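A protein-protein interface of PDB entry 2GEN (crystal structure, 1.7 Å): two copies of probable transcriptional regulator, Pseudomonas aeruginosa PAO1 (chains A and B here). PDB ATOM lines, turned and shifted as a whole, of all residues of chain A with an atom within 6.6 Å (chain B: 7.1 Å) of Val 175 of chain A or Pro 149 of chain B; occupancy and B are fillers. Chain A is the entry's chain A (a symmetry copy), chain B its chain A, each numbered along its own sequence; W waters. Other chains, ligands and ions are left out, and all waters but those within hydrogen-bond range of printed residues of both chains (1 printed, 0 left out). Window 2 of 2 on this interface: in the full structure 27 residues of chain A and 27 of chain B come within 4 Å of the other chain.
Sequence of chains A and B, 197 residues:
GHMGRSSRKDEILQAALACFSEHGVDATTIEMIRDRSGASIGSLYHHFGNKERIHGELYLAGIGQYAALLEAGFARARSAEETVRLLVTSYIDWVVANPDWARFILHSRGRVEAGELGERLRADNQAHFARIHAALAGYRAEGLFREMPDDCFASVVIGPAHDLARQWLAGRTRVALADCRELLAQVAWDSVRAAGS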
ATOM      1  N   LEU A 164      18.711 -11.990 -21.715  1.00  0.00           N
ATOM      2  CA  LEU A 164      19.731 -12.882 -21.122  1.00  0.00           C
ATOM      3  C   LEU A 164      19.283 -14.350 -21.192  1.00  0.00           C
ATOM      4  O   LEU A 164      20.077 -15.227 -21.546  1.00  0.00           O
ATOM      5  CB  LEU A 164      20.035 -12.484 -19.701  1.00  0.00           C
ATOM      6  CG  LEU A 164      21.290 -13.113 -19.049  1.00  0.00           C
ATOM      7  CD1 LEU A 164      22.525 -12.901 -19.950  1.00  0.00           C
ATOM      8  CD2 LEU A 164      21.552 -12.516 -17.684  1.00  0.00           C
ATOM      9  N   TRP A 168      21.369 -17.249 -22.928  1.00  0.00           N
ATOM     10  CA  TRP A 168      21.784 -18.349 -22.059  1.00  0.00           C
ATOM     11  C   TRP A 168      21.313 -19.706 -22.572  1.00  0.00           C
ATOM     12  O   TRP A 168      22.091 -20.672 -22.628  1.00  0.00           O
ATOM     13  CB  TRP A 168      21.277 -18.103 -20.637  1.00  0.00           C
ATOM     14  CG  TRP A 168      21.612 -19.217 -19.686  1.00  0.00           C
ATOM     15  CD1 TRP A 168      22.847 -19.514 -19.158  1.00  0.00           C
ATOM     16  CD2 TRP A 168      20.689 -20.155 -19.115  1.00  0.00           C
ATOM     17  NE1 TRP A 168      22.738 -20.590 -18.301  1.00  0.00           N
ATOM     18  CE2 TRP A 168      21.425 -21.001 -18.259  1.00  0.00           C
ATOM     19  CE3 TRP A 168      19.307 -20.364 -19.248  1.00  0.00           C
ATOM     20  CZ2 TRP A 168      20.821 -22.054 -17.548  1.00  0.00           C
ATOM     21  CZ3 TRP A 168      18.699 -21.411 -18.518  1.00  0.00           C
ATOM     22  CH2 TRP A 168      19.454 -22.235 -17.689  1.00  0.00           C
ATOM     23  N   THR A 173      26.227 -17.308 -23.636  1.00  0.00           N
ATOM     24  CA  THR A 173      26.670 -16.478 -22.502  1.00  0.00           C
ATOM     25  C   THR A 173      27.871 -17.080 -21.743  1.00  0.00           C
ATOM     26  O   THR A 173      28.074 -18.287 -21.751  1.00  0.00           O
ATOM     27  CB  THR A 173      25.536 -16.254 -21.437  1.00  0.00           C
ATOM     28  OG1 THR A 173      25.269 -17.471 -20.724  1.00  0.00           O
ATOM     29  CG2 THR A 173      24.264 -15.747 -22.064  1.00  0.00           C
ATOM     30  N   ARG A 174      28.634 -16.217 -21.073  1.00  0.00           N
ATOM     31  CA  ARG A 174      29.653 -16.674 -20.120  1.00  0.00           C
ATOM     32  C   ARG A 174      29.178 -16.494 -18.670  1.00  0.00           C
ATOM     33  O   ARG A 174      30.016 -16.261 -17.786  1.00  0.00           O
ATOM     34  CB  ARG A 174      30.996 -15.928 -20.279  1.00  0.00           C
ATOM     35  CG  ARG A 174      31.330 -15.315 -21.610  1.00  0.00           C
ATOM     36  CD  ARG A 174      32.183 -14.075 -21.386  1.00  0.00           C
ATOM     37  NE  ARG A 174      31.707 -12.914 -22.137  1.00  0.00           N
ATOM     38  CZ  ARG A 174      32.249 -11.690 -22.094  1.00  0.00           C
ATOM     39  NH1 ARG A 174      33.318 -11.415 -21.343  1.00  0.00           N
ATOM     40  NH2 ARG A 174      31.709 -10.719 -22.815  1.00  0.00           N
ATOM     41  N   VAL A 175      27.863 -16.572 -18.419  1.00  0.00           N
ATOM     42  CA  VAL A 175      27.321 -16.528 -17.047  1.00  0.00           C
ATOM     43  C   VAL A 175      26.228 -17.568 -16.806  1.00  0.00           C
ATOM     44  O   VAL A 175      25.589 -18.009 -17.749  1.00  0.00           O
ATOM     45  CB  VAL A 175      26.745 -15.122 -16.639  1.00  0.00           C
ATOM     46  CG1 VAL A 175      27.739 -14.359 -15.796  1.00  0.00           C
ATOM     47  CG2 VAL A 175      26.287 -14.328 -17.820  1.00  0.00           C
ATOM     48  N   ALA A 176      26.050 -17.985 -15.551  1.00  0.00           N
ATOM     49  CA  ALA A 176      24.927 -18.847 -15.188  1.00  0.00           C
ATOM     50  C   ALA A 176      23.719 -17.913 -15.019  1.00  0.00           C
ATOM     51  O   ALA A 176      23.817 -16.910 -14.297  1.00  0.00           O
ATOM     52  CB  ALA A 176      25.217 -19.588 -13.898  1.00  0.00           C
ATOM     53  N   LEU A 177      22.622 -18.196 -15.721  1.00  0.00           N
ATOM     54  CA  LEU A 177      21.384 -17.386 -15.558  1.00  0.00           C
ATOM     55  C   LEU A 177      20.973 -17.163 -14.098  1.00  0.00           C
ATOM     56  O   LEU A 177      20.681 -16.012 -13.747  1.00  0.00           O
ATOM     57  CB  LEU A 177      20.203 -17.938 -16.380  1.00  0.00           C
ATOM     58  CG  LEU A 177      18.952 -17.038 -16.445  1.00  0.00           C
ATOM     59  CD1 LEU A 177      19.247 -15.670 -17.072  1.00  0.00           C
ATOM     60  CD2 LEU A 177      17.804 -17.723 -17.186  1.00  0.00           C
ATOM     61  N   ALA A 178      20.980 -18.212 -13.251  1.00  0.00           N
ATOM     62  CA  ALA A 178      20.666 -18.064 -11.826  1.00  0.00           C
ATOM     63  C   ALA A 178      21.600 -17.088 -11.128  1.00  0.00           C
ATOM     64  O   ALA A 178      21.178 -16.409 -10.208  1.00  0.00           O
ATOM     65  CB  ALA A 178      20.673 -19.431 -11.084  1.00  0.00           C
ATOM     66  N   ASP A 179      22.862 -16.986 -11.580  1.00  0.00           N
ATOM     67  CA  ASP A 179      23.815 -16.073 -10.942  1.00  0.00           C
ATOM     68  C   ASP A 179      23.533 -14.609 -11.292  1.00  0.00           C
ATOM     69  O   ASP A 179      24.167 -13.731 -10.750  1.00  0.00           O
ATOM     70  CB  ASP A 179      25.282 -16.386 -11.340  1.00  0.00           C
ATOM     71  CG  ASP A 179      25.889 -17.573 -10.578  1.00  0.00           C
ATOM     72  OD1 ASP A 179      25.335 -17.980  -9.531  1.00  0.00           O
ATOM     73  OD2 ASP A 179      26.956 -18.083 -11.054  1.00  0.00           O
ATOM     74  N   CYS A 180      22.611 -14.341 -12.219  1.00  0.00           N
ATOM     75  CA  CYS A 180      22.285 -12.945 -12.544  1.00  0.00           C
ATOM     76  C   CYS A 180      20.890 -12.573 -12.020  1.00  0.00           C
ATOM     77  O   CYS A 180      20.418 -11.478 -12.277  1.00  0.00           O
ATOM     78  CB  CYS A 180      22.285 -12.736 -14.043  1.00  0.00           C
ATOM     79  SG  CYS A 180      23.915 -13.093 -14.779  1.00  0.00           S
ATOM     80  N   LEU A 183      20.957  -9.361  -9.629  1.00  0.00           N
ATOM     81  CA  LEU A 183      21.312  -8.203 -10.416  1.00  0.00           C
ATOM     82  C   LEU A 183      20.138  -7.724 -11.292  1.00  0.00           C
ATOM     83  O   LEU A 183      19.818  -6.518 -11.246  1.00  0.00           O
ATOM     84  CB  LEU A 183      22.497  -8.551 -11.296  1.00  0.00           C
ATOM     85  CG  LEU A 183      23.000  -7.412 -12.147  1.00  0.00           C
ATOM     86  CD1 LEU A 183      23.542  -6.284 -11.269  1.00  0.00           C
ATOM     87  CD2 LEU A 183      24.036  -8.005 -13.085  1.00  0.00           C
ATOM     88  N   ARG B 140      34.839   0.996 -18.117  1.00  0.00           N
ATOM     89  CA  ARG B 140      34.618  -0.007 -17.071  1.00  0.00           C
ATOM     90  C   ARG B 140      35.794   0.110 -16.107  1.00  0.00           C
ATOM     91  O   ARG B 140      35.612   0.136 -14.877  1.00  0.00           O
ATOM     92  CB  ARG B 140      34.560  -1.380 -17.720  1.00  0.00           C
ATOM     93  CG  ARG B 140      33.215  -1.627 -18.416  1.00  0.00           C
ATOM     94  CD  ARG B 140      33.167  -2.881 -19.326  1.00  0.00           C
ATOM     95  NE  ARG B 140      31.780  -3.407 -19.390  1.00  0.00           N
ATOM     96  CZ  ARG B 140      31.350  -4.332 -20.252  1.00  0.00           C
ATOM     97  NH1 ARG B 140      32.149  -4.847 -21.166  1.00  0.00           N
ATOM     98  NH2 ARG B 140      30.101  -4.744 -20.195  1.00  0.00           N
ATOM     99  N   ARG B 146      28.018   0.442 -12.845  1.00  0.00           N
ATOM    100  CA  ARG B 146      27.713  -0.489 -11.762  1.00  0.00           C
ATOM    101  C   ARG B 146      28.299  -1.883 -12.077  1.00  0.00           C
ATOM    102  O   ARG B 146      28.347  -2.327 -13.244  1.00  0.00           O
ATOM    103  CB  ARG B 146      26.199  -0.485 -11.487  1.00  0.00           C
ATOM    104  CG  ARG B 146      25.443  -1.605 -12.114  1.00  0.00           C
ATOM    105  CD  ARG B 146      23.942  -1.657 -11.643  1.00  0.00           C
ATOM    106  NE  ARG B 146      23.794  -2.575 -10.514  1.00  0.00           N
ATOM    107  CZ  ARG B 146      22.762  -2.616  -9.664  1.00  0.00           C
ATOM    108  NH1 ARG B 146      21.723  -1.767  -9.772  1.00  0.00           N
ATOM    109  NH2 ARG B 146      22.788  -3.523  -8.686  1.00  0.00           N
ATOM    110  N   GLU B 147      28.767  -2.581 -11.045  1.00  0.00           N
ATOM    111  CA  GLU B 147      29.456  -3.880 -11.244  1.00  0.00           C
ATOM    112  C   GLU B 147      28.482  -4.962 -11.704  1.00  0.00           C
ATOM    113  O   GLU B 147      27.464  -5.208 -11.048  1.00  0.00           O
ATOM    114  CB  GLU B 147      30.170  -4.356  -9.959  1.00  0.00           C
ATOM    115  CG  GLU B 147      30.970  -3.273  -9.190  1.00  0.00           C
ATOM    116  CD  GLU B 147      31.985  -3.875  -8.205  1.00  0.00           C
ATOM    117  OE1 GLU B 147      31.640  -4.865  -7.501  1.00  0.00           O
ATOM    118  OE2 GLU B 147      33.141  -3.367  -8.148  1.00  0.00           O
ATOM    119  N   MET B 148      28.787  -5.578 -12.837  1.00  0.00           N
ATOM    120  CA  MET B 148      28.049  -6.714 -13.350  1.00  0.00           C
ATOM    121  C   MET B 148      28.856  -7.452 -14.413  1.00  0.00           C
ATOM    122  O   MET B 148      29.756  -6.844 -15.036  1.00  0.00           O
ATOM    123  CB  MET B 148      26.661  -6.274 -13.893  1.00  0.00           C
ATOM    124  CG  MET B 148      26.698  -5.592 -15.176  1.00  0.00           C
ATOM    125  SD  MET B 148      24.860  -4.865 -15.600  1.00  0.00           S
ATOM    126  CE  MET B 148      24.916  -3.285 -14.700  1.00  0.00           C
ATOM    127  N   PRO B 149      28.557  -8.741 -14.642  1.00  0.00           N
ATOM    128  CA  PRO B 149      29.173  -9.504 -15.735  1.00  0.00           C
ATOM    129  C   PRO B 149      28.915  -8.870 -17.098  1.00  0.00           C
ATOM    130  O   PRO B 149      27.857  -8.274 -17.305  1.00  0.00           O
ATOM    131  CB  PRO B 149      28.497 -10.866 -15.655  1.00  0.00           C
ATOM    132  CG  PRO B 149      27.953 -10.948 -14.253  1.00  0.00           C
ATOM    133  CD  PRO B 149      27.633  -9.571 -13.838  1.00  0.00           C
ATOM    134  N   ASP B 150      29.873  -8.989 -18.005  1.00  0.00           N
ATOM    135  CA  ASP B 150      29.759  -8.379 -19.357  1.00  0.00           C
ATOM    136  C   ASP B 150      28.461  -8.799 -20.060  1.00  0.00           C
ATOM    137  O   ASP B 150      27.788  -7.944 -20.693  1.00  0.00           O
ATOM    138  CB  ASP B 150      30.953  -8.789 -20.246  1.00  0.00           C
ATOM    139  CG  ASP B 150      32.269  -8.127 -19.840  1.00  0.00           C
ATOM    140  OD1 ASP B 150      32.286  -7.194 -19.009  1.00  0.00           O
ATOM    141  OD2 ASP B 150      33.330  -8.575 -20.361  1.00  0.00           O
ATOM    142  N   ASP B 151      28.078 -10.084 -19.930  1.00  0.00           N
ATOM    143  CA  ASP B 151      26.827 -10.571 -20.548  1.00  0.00           C
ATOM    144  C   ASP B 151      25.588  -9.939 -19.952  1.00  0.00           C
ATOM    145  O   ASP B 151      24.614  -9.690 -20.700  1.00  0.00           O
ATOM    146  CB  ASP B 151      26.633 -12.082 -20.453  1.00  0.00           C
ATOM    147  CG  ASP B 151      27.698 -12.875 -21.168  1.00  0.00           C
ATOM    148  OD1 ASP B 151      28.011 -12.599 -22.350  1.00  0.00           O
ATOM    149  OD2 ASP B 151      28.194 -13.826 -20.528  1.00  0.00           O
ATOM    150  N   CYS B 152      25.607  -9.688 -18.637  1.00  0.00           N
ATOM    151  CA  CYS B 152      24.505  -8.978 -17.962  1.00  0.00           C
ATOM    152  C   CYS B 152      24.393  -7.540 -18.462  1.00  0.00           C
ATOM    153  O   CYS B 152      23.307  -7.087 -18.867  1.00  0.00           O
ATOM    154  CB  CYS B 152      24.737  -8.914 -16.471  1.00  0.00           C
ATOM    155  SG  CYS B 152      24.551 -10.491 -15.743  1.00  0.00           S
ATOM    156  N   PHE B 153      25.523  -6.821 -18.419  1.00  0.00           N
ATOM    157  CA  PHE B 153      25.595  -5.470 -19.009  1.00  0.00           C
ATOM    158  C   PHE B 153      24.985  -5.450 -20.424  1.00  0.00           C
ATOM    159  O   PHE B 153      24.147  -4.575 -20.704  1.00  0.00           O
ATOM    160  CB  PHE B 153      27.041  -4.945 -18.995  1.00  0.00           C
ATOM    161  CG  PHE B 153      27.205  -3.531 -19.483  1.00  0.00           C
ATOM    162  CD1 PHE B 153      27.473  -2.511 -18.572  1.00  0.00           C
ATOM    163  CD2 PHE B 153      27.144  -3.225 -20.833  1.00  0.00           C
ATOM    164  CE1 PHE B 153      27.674  -1.196 -18.968  1.00  0.00           C
ATOM    165  CE2 PHE B 153      27.377  -1.879 -21.261  1.00  0.00           C
ATOM    166  CZ  PHE B 153      27.605  -0.860 -20.303  1.00  0.00           C
ATOM    167  N   ALA B 154      25.384  -6.371 -21.297  1.00  0.00           N
ATOM    168  CA  ALA B 154      24.872  -6.394 -22.685  1.00  0.00           C
ATOM    169  C   ALA B 154      23.341  -6.456 -22.722  1.00  0.00           C
ATOM    170  O   ALA B 154      22.684  -5.656 -23.416  1.00  0.00           O
ATOM    171  CB  ALA B 154      25.477  -7.555 -23.477  1.00  0.00           C
ATOM    172  N   SER B 155      22.790  -7.400 -21.953  1.00  0.00           N
ATOM    173  CA  SER B 155      21.316  -7.594 -21.879  1.00  0.00           C
ATOM    174  C   SER B 155      20.598  -6.483 -21.162  1.00  0.00           C
ATOM    175  O   SER B 155      19.429  -6.184 -21.553  1.00  0.00           O
ATOM    176  CB  SER B 155      20.969  -8.936 -21.198  1.00  0.00           C
ATOM    177  OG  SER B 155      21.235  -9.986 -22.112  1.00  0.00           O
HETATM  178  O   HOH W   1      29.154 -14.031 -24.038  1.00  0.00           O
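The side-chain carboxylate (OD2) of Asp 150 of chain B lies within salt-bridge range of the guanidinium group (NH1) of Arg 174 of chain A (3.0 Å). OD1 of Asp 151 of chain B is in salt-bridge range of NE of Arg 174 of chain A (3.7 Å). The side-chain carboxylate (OD2) of Asp 151 of chain B lies close to the backbone NH (N) of Val 175 of chain A (3.5 Å). The side-chain hydroxyl (OG) of Ser 155 of chain B sits at hydrogen-bond distance from the backbone NH (N) of Leu 164 of chain A. SG of Cys 180 of chain A lies close to SG of Cys 152 of chain B, 2.8 Å away.
The guanidinium group (NH1) of Arg 140 of chain B lies within salt-bridge range of the side-chain carboxylate (OD1) of Asp 150 of chain B, 3.2 Å away. The side-chain sulfur (SD) of Met 148 of chain B lies within hydrogen-bond range of the backbone NH (N) of Phe 153 of chain B, at 3.5 Å. The side-chain hydroxyl (OG1) of Thr 173 of chain A lies within hydrogen-bond range of the backbone carbonyl oxygen (O) of Val 175 of chain A (3.0 Å).
Of the 11 printed residues of chain B, 7 touch a printed residue of chain A.
Water W1 bridges the side-chain carboxylate of Asp 151 of chain B and the guanidinium group of Arg 174 of chain A.
Among the printed residues, merely in contact across the chains: Leu 164 of chain A with Asp 151 of chain B (3.9 Å), Thr 173 of chain A with Asp 151 of chain B (3.5 Å), Val 175 of chain A with Pro 149 of chain B (3.6 Å), Leu 183 of chain A with Arg 146 of chain B (3.8 Å), Leu 183 of chain A with Met 148 of chain B (3.2 Å), Leu 183 of chain A with Pro 149 of chain B (3.99 Å) and Leu 183 of chain A with Cys 152 of chain B (3.6 Å).
No position is printed for both chains.
Of the printed residues of chain B, Thr 173 of chain A touches Asp 151. Of the printed residues of chain B, Arg 174 of chain A touches Asp 150 (3.0 Å) and Asp 151 (2.5 Å). Of chain B, only Pro 149 and Asp 151 come within 4 Å of Val 175 of chain A. Of the printed residues of chain B, Cys 180 of chain A touches Cys 152. Of the printed residues of chain A, Met 148 of chain B touches Leu 183 (3.2 Å). Printed residues of chain A within 4 Å of Ser 155 of chain B: Leu 164 (3.2 Å). The nearest residue of chain B that does not touch Val 175 of chain A is Cys 152 of chain B (4.7 Å). The nearest printed residue of chain B that does not touch Thr 173 of chain A is Ser 155 of chain B (6.5 Å).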
